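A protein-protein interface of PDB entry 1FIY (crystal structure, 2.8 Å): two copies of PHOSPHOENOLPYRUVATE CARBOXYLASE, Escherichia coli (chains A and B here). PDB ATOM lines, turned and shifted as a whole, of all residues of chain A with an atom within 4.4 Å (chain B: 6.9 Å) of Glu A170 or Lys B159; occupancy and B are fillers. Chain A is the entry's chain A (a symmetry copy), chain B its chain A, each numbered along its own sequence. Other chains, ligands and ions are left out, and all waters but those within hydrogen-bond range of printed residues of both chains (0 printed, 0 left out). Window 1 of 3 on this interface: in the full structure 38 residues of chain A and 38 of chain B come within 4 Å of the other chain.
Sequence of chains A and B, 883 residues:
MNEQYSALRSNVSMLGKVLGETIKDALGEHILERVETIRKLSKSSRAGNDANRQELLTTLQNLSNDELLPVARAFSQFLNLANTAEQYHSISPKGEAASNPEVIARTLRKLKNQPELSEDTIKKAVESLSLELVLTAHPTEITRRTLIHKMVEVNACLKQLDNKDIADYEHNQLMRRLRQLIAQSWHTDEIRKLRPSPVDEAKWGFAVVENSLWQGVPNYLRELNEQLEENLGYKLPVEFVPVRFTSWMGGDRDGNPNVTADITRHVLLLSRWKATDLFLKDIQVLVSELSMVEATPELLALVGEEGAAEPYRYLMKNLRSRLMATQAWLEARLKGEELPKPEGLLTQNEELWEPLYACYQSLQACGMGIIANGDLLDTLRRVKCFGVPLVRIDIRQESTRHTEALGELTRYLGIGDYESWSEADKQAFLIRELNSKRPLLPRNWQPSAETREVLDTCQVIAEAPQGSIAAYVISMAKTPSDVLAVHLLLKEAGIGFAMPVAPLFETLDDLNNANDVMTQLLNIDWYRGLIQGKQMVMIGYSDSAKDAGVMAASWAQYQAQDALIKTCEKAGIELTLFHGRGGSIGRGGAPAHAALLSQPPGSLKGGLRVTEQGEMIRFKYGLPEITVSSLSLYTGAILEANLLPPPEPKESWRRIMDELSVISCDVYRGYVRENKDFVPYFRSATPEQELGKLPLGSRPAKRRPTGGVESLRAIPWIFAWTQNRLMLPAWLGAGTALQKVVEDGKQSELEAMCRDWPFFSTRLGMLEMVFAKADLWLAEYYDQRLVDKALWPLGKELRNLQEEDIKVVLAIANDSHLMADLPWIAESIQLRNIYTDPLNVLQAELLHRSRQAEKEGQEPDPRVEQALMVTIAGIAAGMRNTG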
ATOM      1  N   ILE A 166      -5.459  -8.091 -23.923  1.00  0.00           N
ATOM      2  CA  ILE A 166      -6.330  -8.442 -22.796  1.00  0.00           C
ATOM      3  C   ILE A 166      -7.469  -7.409 -22.874  1.00  0.00           C
ATOM      4  O   ILE A 166      -7.202  -6.225 -23.008  1.00  0.00           O
ATOM      5  CB  ILE A 166      -5.853  -8.649 -21.393  1.00  0.00           C
ATOM      6  CG1 ILE A 166      -5.089  -7.481 -20.772  1.00  0.00           C
ATOM      7  CG2 ILE A 166      -5.030  -9.935 -21.265  1.00  0.00           C
ATOM      8  CD1 ILE A 166      -5.068  -7.578 -19.255  1.00  0.00           C
ATOM      9  N   ALA A 167      -8.672  -7.956 -22.860  1.00  0.00           N
ATOM     10  CA  ALA A 167      -9.855  -7.089 -22.909  1.00  0.00           C
ATOM     11  C   ALA A 167      -9.691  -6.038 -21.824  1.00  0.00           C
ATOM     12  O   ALA A 167      -9.291  -6.356 -20.688  1.00  0.00           O
ATOM     13  CB  ALA A 167     -11.080  -7.959 -22.689  1.00  0.00           C
ATOM     14  N   ASP A 168      -9.990  -4.787 -22.122  1.00  0.00           N
ATOM     15  CA  ASP A 168      -9.856  -3.731 -21.130  1.00  0.00           C
ATOM     16  C   ASP A 168     -10.526  -4.042 -19.804  1.00  0.00           C
ATOM     17  O   ASP A 168      -9.937  -3.680 -18.776  1.00  0.00           O
ATOM     18  CB  ASP A 168     -10.325  -2.388 -21.666  1.00  0.00           C
ATOM     19  CG  ASP A 168     -11.645  -2.443 -22.392  1.00  0.00           C
ATOM     20  OD1 ASP A 168     -12.211  -3.551 -22.544  1.00  0.00           O
ATOM     21  OD2 ASP A 168     -12.110  -1.357 -22.812  1.00  0.00           O
ATOM     22  N   TYR A 169     -11.691  -4.685 -19.764  1.00  0.00           N
ATOM     23  CA  TYR A 169     -12.356  -5.016 -18.521  1.00  0.00           C
ATOM     24  C   TYR A 169     -11.502  -5.950 -17.669  1.00  0.00           C
ATOM     25  O   TYR A 169     -11.440  -5.764 -16.455  1.00  0.00           O
ATOM     26  CB  TYR A 169     -13.748  -5.578 -18.678  1.00  0.00           C
ATOM     27  CG  TYR A 169     -13.987  -6.667 -19.677  1.00  0.00           C
ATOM     28  CD1 TYR A 169     -13.960  -6.395 -21.042  1.00  0.00           C
ATOM     29  CD2 TYR A 169     -14.259  -7.970 -19.284  1.00  0.00           C
ATOM     30  CE1 TYR A 169     -14.188  -7.391 -21.972  1.00  0.00           C
ATOM     31  CE2 TYR A 169     -14.485  -8.976 -20.207  1.00  0.00           C
ATOM     32  CZ  TYR A 169     -14.444  -8.674 -21.546  1.00  0.00           C
ATOM     33  OH  TYR A 169     -14.657  -9.645 -22.487  1.00  0.00           O
ATOM     34  N   GLU A 170     -10.844  -6.919 -18.308  1.00  0.00           N
ATOM     35  CA  GLU A 170      -9.965  -7.824 -17.569  1.00  0.00           C
ATOM     36  C   GLU A 170      -8.793  -7.026 -16.965  1.00  0.00           C
ATOM     37  O   GLU A 170      -8.410  -7.208 -15.805  1.00  0.00           O
ATOM     38  CB  GLU A 170      -9.405  -8.923 -18.440  1.00  0.00           C
ATOM     39  CG  GLU A 170     -10.341  -9.613 -19.412  1.00  0.00           C
ATOM     40  CD  GLU A 170      -9.540 -10.594 -20.272  1.00  0.00           C
ATOM     41  OE1 GLU A 170      -9.163 -11.664 -19.756  1.00  0.00           O
ATOM     42  OE2 GLU A 170      -9.283 -10.277 -21.452  1.00  0.00           O
ATOM     43  N   HIS A 171      -8.245  -6.111 -17.767  1.00  0.00           N
ATOM     44  CA  HIS A 171      -7.146  -5.273 -17.317  1.00  0.00           C
ATOM     45  C   HIS A 171      -7.528  -4.464 -16.093  1.00  0.00           C
ATOM     46  O   HIS A 171      -6.771  -4.326 -15.138  1.00  0.00           O
ATOM     47  CB  HIS A 171      -6.709  -4.349 -18.453  1.00  0.00           C
ATOM     48  CG  HIS A 171      -5.446  -3.603 -18.165  1.00  0.00           C
ATOM     49  ND1 HIS A 171      -5.437  -2.409 -17.478  1.00  0.00           N
ATOM     50  CD2 HIS A 171      -4.156  -3.885 -18.475  1.00  0.00           C
ATOM     51  CE1 HIS A 171      -4.197  -1.977 -17.373  1.00  0.00           C
ATOM     52  NE2 HIS A 171      -3.402  -2.856 -17.962  1.00  0.00           N
ATOM     53  N   ASN A 172      -8.731  -3.913 -16.105  1.00  0.00           N
ATOM     54  CA  ASN A 172      -9.282  -3.113 -15.026  1.00  0.00           C
ATOM     55  C   ASN A 172      -9.406  -3.962 -13.761  1.00  0.00           C
ATOM     56  O   ASN A 172      -9.101  -3.526 -12.652  1.00  0.00           O
ATOM     57  CB  ASN A 172     -10.635  -2.548 -15.467  1.00  0.00           C
ATOM     58  CG  ASN A 172     -11.229  -1.522 -14.526  1.00  0.00           C
ATOM     59  OD1 ASN A 172     -11.838  -1.832 -13.493  1.00  0.00           O
ATOM     60  ND2 ASN A 172     -11.068  -0.240 -14.872  1.00  0.00           N
ATOM     61  N   GLN A 173      -9.864  -5.199 -13.951  1.00  0.00           N
ATOM     62  CA  GLN A 173     -10.031  -6.144 -12.852  1.00  0.00           C
ATOM     63  C   GLN A 173      -8.667  -6.467 -12.233  1.00  0.00           C
ATOM     64  O   GLN A 173      -8.457  -6.398 -11.018  1.00  0.00           O
ATOM     65  CB  GLN A 173     -10.739  -7.400 -13.365  1.00  0.00           C
ATOM     66  CG  GLN A 173     -12.225  -7.276 -13.567  1.00  0.00           C
ATOM     67  CD  GLN A 173     -12.866  -8.320 -14.449  1.00  0.00           C
ATOM     68  OE1 GLN A 173     -12.391  -9.447 -14.635  1.00  0.00           O
ATOM     69  NE2 GLN A 173     -14.016  -7.988 -15.053  1.00  0.00           N
ATOM     70  N   LEU A 174      -7.716  -6.796 -13.124  1.00  0.00           N
ATOM     71  CA  LEU A 174      -6.350  -7.117 -12.707  1.00  0.00           C
ATOM     72  C   LEU A 174      -5.741  -5.960 -11.939  1.00  0.00           C
ATOM     73  O   LEU A 174      -5.294  -6.075 -10.794  1.00  0.00           O
ATOM     74  CB  LEU A 174      -5.523  -7.517 -13.919  1.00  0.00           C
ATOM     75  CG  LEU A 174      -5.803  -8.921 -14.470  1.00  0.00           C
ATOM     76  CD1 LEU A 174      -5.005  -9.196 -15.728  1.00  0.00           C
ATOM     77  CD2 LEU A 174      -5.518  -9.974 -13.416  1.00  0.00           C
ATOM     78  N   TYR B  88     -16.905 -21.606 -23.218  1.00  0.00           N
ATOM     79  CA  TYR B  88     -15.687 -20.812 -23.085  1.00  0.00           C
ATOM     80  C   TYR B  88     -15.774 -19.593 -23.996  1.00  0.00           C
ATOM     81  O   TYR B  88     -15.527 -18.442 -23.650  1.00  0.00           O
ATOM     82  CB  TYR B  88     -14.405 -21.652 -23.387  1.00  0.00           C
ATOM     83  CG  TYR B  88     -13.243 -20.666 -23.516  1.00  0.00           C
ATOM     84  CD1 TYR B  88     -12.832 -19.952 -22.394  1.00  0.00           C
ATOM     85  CD2 TYR B  88     -12.659 -20.392 -24.737  1.00  0.00           C
ATOM     86  CE1 TYR B  88     -11.835 -19.011 -22.520  1.00  0.00           C
ATOM     87  CE2 TYR B  88     -11.663 -19.450 -24.858  1.00  0.00           C
ATOM     88  CZ  TYR B  88     -11.257 -18.766 -23.749  1.00  0.00           C
ATOM     89  OH  TYR B  88     -10.259 -17.822 -23.824  1.00  0.00           O
ATOM     90  N   SER B  92     -15.371 -15.486 -23.294  1.00  0.00           N
ATOM     91  CA  SER B  92     -14.098 -15.065 -23.854  1.00  0.00           C
ATOM     92  C   SER B  92     -14.240 -13.725 -24.552  1.00  0.00           C
ATOM     93  O   SER B  92     -15.003 -13.578 -25.508  1.00  0.00           O
ATOM     94  CB  SER B  92     -13.605 -16.110 -24.861  1.00  0.00           C
ATOM     95  OG  SER B  92     -13.251 -15.475 -26.073  1.00  0.00           O
ATOM     96  N   PRO B  93     -13.458 -12.741 -24.123  1.00  0.00           N
ATOM     97  CA  PRO B  93     -13.472 -11.412 -24.705  1.00  0.00           C
ATOM     98  C   PRO B  93     -13.301 -11.375 -26.207  1.00  0.00           C
ATOM     99  O   PRO B  93     -13.768 -10.399 -26.827  1.00  0.00           O
ATOM    100  CB  PRO B  93     -12.378 -10.667 -23.959  1.00  0.00           C
ATOM    101  CG  PRO B  93     -12.226 -11.397 -22.669  1.00  0.00           C
ATOM    102  CD  PRO B  93     -12.506 -12.840 -22.994  1.00  0.00           C
ATOM    103  N   LYS B  94     -12.672 -12.347 -26.859  1.00  0.00           N
ATOM    104  CA  LYS B  94     -12.556 -12.369 -28.314  1.00  0.00           C
ATOM    105  C   LYS B  94     -13.499 -13.482 -28.803  1.00  0.00           C
ATOM    106  O   LYS B  94     -13.087 -14.512 -29.316  1.00  0.00           O
ATOM    107  CB  LYS B  94     -11.158 -12.640 -28.828  1.00  0.00           C
ATOM    108  CG  LYS B  94     -11.040 -12.704 -30.353  1.00  0.00           C
ATOM    109  CD  LYS B  94      -9.804 -13.475 -30.807  1.00  0.00           C
ATOM    110  CE  LYS B  94      -9.791 -13.699 -32.318  1.00  0.00           C
ATOM    111  NZ  LYS B  94      -8.529 -13.168 -32.937  1.00  0.00           N
ATOM    112  N   PRO B 101     -18.672  -5.797 -18.921  1.00  0.00           N
ATOM    113  CA  PRO B 101     -19.476  -4.789 -18.277  1.00  0.00           C
ATOM    114  C   PRO B 101     -20.253  -3.830 -19.140  1.00  0.00           C
ATOM    115  O   PRO B 101     -21.066  -3.065 -18.570  1.00  0.00           O
ATOM    116  CB  PRO B 101     -18.472  -4.041 -17.401  1.00  0.00           C
ATOM    117  CG  PRO B 101     -17.404  -5.033 -17.122  1.00  0.00           C
ATOM    118  CD  PRO B 101     -17.298  -5.876 -18.364  1.00  0.00           C
ATOM    119  N   GLU B 153     -11.824 -25.855 -14.119  1.00  0.00           N
ATOM    120  CA  GLU B 153     -10.466 -26.144 -14.484  1.00  0.00           C
ATOM    121  C   GLU B 153     -10.311 -26.282 -15.986  1.00  0.00           C
ATOM    122  O   GLU B 153      -9.452 -25.598 -16.559  1.00  0.00           O
ATOM    123  CB  GLU B 153      -9.976 -27.417 -13.781  1.00  0.00           C
ATOM    124  CG  GLU B 153      -8.762 -27.145 -12.895  1.00  0.00           C
ATOM    125  CD  GLU B 153      -7.795 -28.311 -12.845  1.00  0.00           C
ATOM    126  OE1 GLU B 153      -8.258 -29.477 -12.798  1.00  0.00           O
ATOM    127  OE2 GLU B 153      -6.568 -28.037 -12.855  1.00  0.00           O
ATOM    128  N   VAL B 154     -11.147 -27.085 -16.640  1.00  0.00           N
ATOM    129  CA  VAL B 154     -11.040 -27.201 -18.099  1.00  0.00           C
ATOM    130  C   VAL B 154     -11.104 -25.843 -18.791  1.00  0.00           C
ATOM    131  O   VAL B 154     -10.361 -25.590 -19.734  1.00  0.00           O
ATOM    132  CB  VAL B 154     -12.086 -28.124 -18.710  1.00  0.00           C
ATOM    133  CG1 VAL B 154     -11.992 -28.076 -20.234  1.00  0.00           C
ATOM    134  CG2 VAL B 154     -11.876 -29.536 -18.191  1.00  0.00           C
ATOM    135  N   ASN B 155     -11.983 -24.973 -18.325  1.00  0.00           N
ATOM    136  CA  ASN B 155     -12.175 -23.626 -18.799  1.00  0.00           C
ATOM    137  C   ASN B 155     -10.966 -22.749 -18.493  1.00  0.00           C
ATOM    138  O   ASN B 155     -10.686 -21.819 -19.251  1.00  0.00           O
ATOM    139  CB  ASN B 155     -13.382 -23.000 -18.089  1.00  0.00           C
ATOM    140  CG  ASN B 155     -13.751 -21.632 -18.609  1.00  0.00           C
ATOM    141  OD1 ASN B 155     -14.375 -21.579 -19.670  1.00  0.00           O
ATOM    142  ND2 ASN B 155     -13.405 -20.567 -17.916  1.00  0.00           N
ATOM    143  N   ALA B 156     -10.272 -23.013 -17.386  1.00  0.00           N
ATOM    144  CA  ALA B 156      -9.089 -22.205 -17.057  1.00  0.00           C
ATOM    145  C   ALA B 156      -7.987 -22.577 -18.052  1.00  0.00           C
ATOM    146  O   ALA B 156      -7.350 -21.705 -18.634  1.00  0.00           O
ATOM    147  CB  ALA B 156      -8.626 -22.416 -15.636  1.00  0.00           C
ATOM    148  N   CYS B 157      -7.836 -23.877 -18.292  1.00  0.00           N
ATOM    149  CA  CYS B 157      -6.830 -24.318 -19.249  1.00  0.00           C
ATOM    150  C   CYS B 157      -7.038 -23.688 -20.607  1.00  0.00           C
ATOM    151  O   CYS B 157      -6.075 -23.229 -21.237  1.00  0.00           O
ATOM    152  CB  CYS B 157      -6.720 -25.845 -19.252  1.00  0.00           C
ATOM    153  SG  CYS B 157      -5.550 -26.399 -17.937  1.00  0.00           S
ATOM    154  N   LEU B 158      -8.273 -23.583 -21.090  1.00  0.00           N
ATOM    155  CA  LEU B 158      -8.606 -22.964 -22.356  1.00  0.00           C
ATOM    156  C   LEU B 158      -8.322 -21.466 -22.327  1.00  0.00           C
ATOM    157  O   LEU B 158      -7.922 -20.868 -23.322  1.00  0.00           O
ATOM    158  CB  LEU B 158     -10.076 -23.168 -22.692  1.00  0.00           C
ATOM    159  CG  LEU B 158     -10.553 -24.583 -22.966  1.00  0.00           C
ATOM    160  CD1 LEU B 158     -12.014 -24.582 -23.418  1.00  0.00           C
ATOM    161  CD2 LEU B 158      -9.675 -25.283 -23.984  1.00  0.00           C
ATOM    162  N   LYS B 159      -8.546 -20.834 -21.183  1.00  0.00           N
ATOM    163  CA  LYS B 159      -8.267 -19.393 -21.103  1.00  0.00           C
ATOM    164  C   LYS B 159      -6.777 -19.167 -21.350  1.00  0.00           C
ATOM    165  O   LYS B 159      -6.363 -18.390 -22.209  1.00  0.00           O
ATOM    166  CB  LYS B 159      -8.720 -18.857 -19.757  1.00  0.00           C
ATOM    167  CG  LYS B 159      -8.388 -17.418 -19.465  1.00  0.00           C
ATOM    168  CD  LYS B 159      -9.521 -16.688 -18.769  1.00  0.00           C
ATOM    169  CE  LYS B 159      -9.076 -15.292 -18.351  1.00  0.00           C
ATOM    170  NZ  LYS B 159      -9.821 -14.799 -17.152  1.00  0.00           N
ATOM    171  N   GLN B 160      -5.929 -19.882 -20.612  1.00  0.00           N
ATOM    172  CA  GLN B 160      -4.490 -19.770 -20.739  1.00  0.00           C
ATOM    173  C   GLN B 160      -3.946 -20.101 -22.117  1.00  0.00           C
ATOM    174  O   GLN B 160      -2.980 -19.468 -22.588  1.00  0.00           O
ATOM    175  CB  GLN B 160      -3.813 -20.627 -19.665  1.00  0.00           C
ATOM    176  CG  GLN B 160      -3.470 -19.784 -18.434  1.00  0.00           C
ATOM    177  CD  GLN B 160      -3.570 -20.631 -17.179  1.00  0.00           C
ATOM    178  OE1 GLN B 160      -4.677 -20.924 -16.733  1.00  0.00           O
ATOM    179  NE2 GLN B 160      -2.442 -21.040 -16.616  1.00  0.00           N
ATOM    180  N   LEU B 161      -4.536 -21.064 -22.819  1.00  0.00           N
ATOM    181  CA  LEU B 161      -4.074 -21.413 -24.158  1.00  0.00           C
ATOM    182  C   LEU B 161      -4.445 -20.349 -25.174  1.00  0.00           C
ATOM    183  O   LEU B 161      -3.814 -20.206 -26.227  1.00  0.00           O
ATOM    184  CB  LEU B 161      -4.576 -22.802 -24.526  1.00  0.00           C
ATOM    185  CG  LEU B 161      -3.939 -23.957 -23.738  1.00  0.00           C
ATOM    186  CD1 LEU B 161      -4.649 -25.275 -23.977  1.00  0.00           C
ATOM    187  CD2 LEU B 161      -2.465 -24.092 -24.081  1.00  0.00           C
ATOM    188  N   ASP B 162      -5.430 -19.509 -24.879  1.00  0.00           N
ATOM    189  CA  ASP B 162      -5.914 -18.448 -25.727  1.00  0.00           C
ATOM    190  C   ASP B 162      -4.907 -17.325 -25.924  1.00  0.00           C
ATOM    191  O   ASP B 162      -5.042 -16.549 -26.881  1.00  0.00           O
ATOM    192  CB  ASP B 162      -7.180 -17.828 -25.149  1.00  0.00           C
ATOM    193  CG  ASP B 162      -8.310 -17.557 -26.098  1.00  0.00           C
ATOM    194  OD1 ASP B 162      -8.536 -18.302 -27.066  1.00  0.00           O
ATOM    195  OD2 ASP B 162      -9.030 -16.557 -25.853  1.00  0.00           O
ATOM    196  N   ASN B 163      -3.947 -17.215 -25.027  1.00  0.00           N
ATOM    197  CA  ASN B 163      -2.930 -16.175 -25.114  1.00  0.00           C
ATOM    198  C   ASN B 163      -1.935 -16.457 -26.235  1.00  0.00           C
ATOM    199  O   ASN B 163      -1.208 -17.446 -26.176  1.00  0.00           O
ATOM    200  CB  ASN B 163      -2.204 -16.069 -23.778  1.00  0.00           C
ATOM    201  CG  ASN B 163      -1.014 -15.148 -23.764  1.00  0.00           C
ATOM    202  OD1 ASN B 163      -0.146 -15.268 -22.888  1.00  0.00           O
ATOM    203  ND2 ASN B 163      -0.937 -14.212 -24.701  1.00  0.00           N
ATOM    204  N   LEU B 174       0.474 -26.642 -20.298  1.00  0.00           N
ATOM    205  CA  LEU B 174      -0.980 -26.487 -20.358  1.00  0.00           C
ATOM    206  C   LEU B 174      -1.621 -27.703 -20.999  1.00  0.00           C
ATOM    207  O   LEU B 174      -2.489 -28.378 -20.439  1.00  0.00           O
ATOM    208  CB  LEU B 174      -1.330 -25.192 -21.076  1.00  0.00           C
ATOM    209  CG  LEU B 174      -1.115 -23.911 -20.260  1.00  0.00           C
ATOM    210  CD1 LEU B 174      -1.398 -22.671 -21.083  1.00  0.00           C
ATOM    211  CD2 LEU B 174      -1.971 -23.928 -19.007  1.00  0.00           C
ATOM    212  N   GLU B 625     -17.864 -16.238 -14.198  1.00  0.00           N
ATOM    213  CA  GLU B 625     -18.082 -15.205 -15.226  1.00  0.00           C
ATOM    214  C   GLU B 625     -19.452 -15.392 -15.861  1.00  0.00           C
ATOM    215  O   GLU B 625     -20.148 -14.393 -16.088  1.00  0.00           O
ATOM    216  CB  GLU B 625     -17.005 -15.156 -16.286  1.00  0.00           C
ATOM    217  CG  GLU B 625     -15.605 -14.979 -15.722  1.00  0.00           C
ATOM    218  CD  GLU B 625     -14.943 -16.318 -15.451  1.00  0.00           C
ATOM    219  OE1 GLU B 625     -15.250 -16.972 -14.424  1.00  0.00           O
ATOM    220  OE2 GLU B 625     -14.105 -16.735 -16.289  1.00  0.00           O
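OE2 of Glu A170 sits at hydrogen-bond distance from N of Ala A167, 2.8 Å away.
Among the printed residues, merely in contact across the chains: Ala A167 with Pro B93 (3.3 Å), Tyr A169 with Pro B93 (2.9 Å), Tyr A169 with Pro B101 (3.6 Å), Glu A170 with Pro B93 (3.4 Å) and Glu A170 with Lys B159 (3.9 Å).
Of the printed residues of chain B, Ala A167 touches Pro B93 (3.3 Å). Printed residues of chain B within 4 Å of Tyr A169: Pro B93 (2.9 Å) and Pro B101 (3.6 Å). Of the printed residues of chain A, Pro B93 touches Ala A167 (3.3 Å), Tyr A169 (2.9 Å) and Glu A170 (3.4 Å). Of the printed residues of chain A, Pro B101 touches Tyr A169. Glu B625 touches none of the printed residues of chain A. The nearest printed residue of chain A that does not touch Lys B159 is Gln A173 (6.4 Å). The nearest printed residue of chain B that does not touch Tyr A169 is Ser B92 (4.6 Å).
Printed residues of chain A that touch a printed residue of chain B: Ala A167, Tyr A169 and Glu A170. Printed residues of chain B that touch a printed residue of chain A: Pro B93, Pro B101 and Lys B159. Along chain B the printed residues that touch a printed residue of chain A span positions 93 to 159. Among the printed residues, 5 pairs touch across the chains.
1 position is printed for both chains. Of the 5 pairs that touch across the chains among the printed residues, none has its exchanged pair printed and touching as well.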
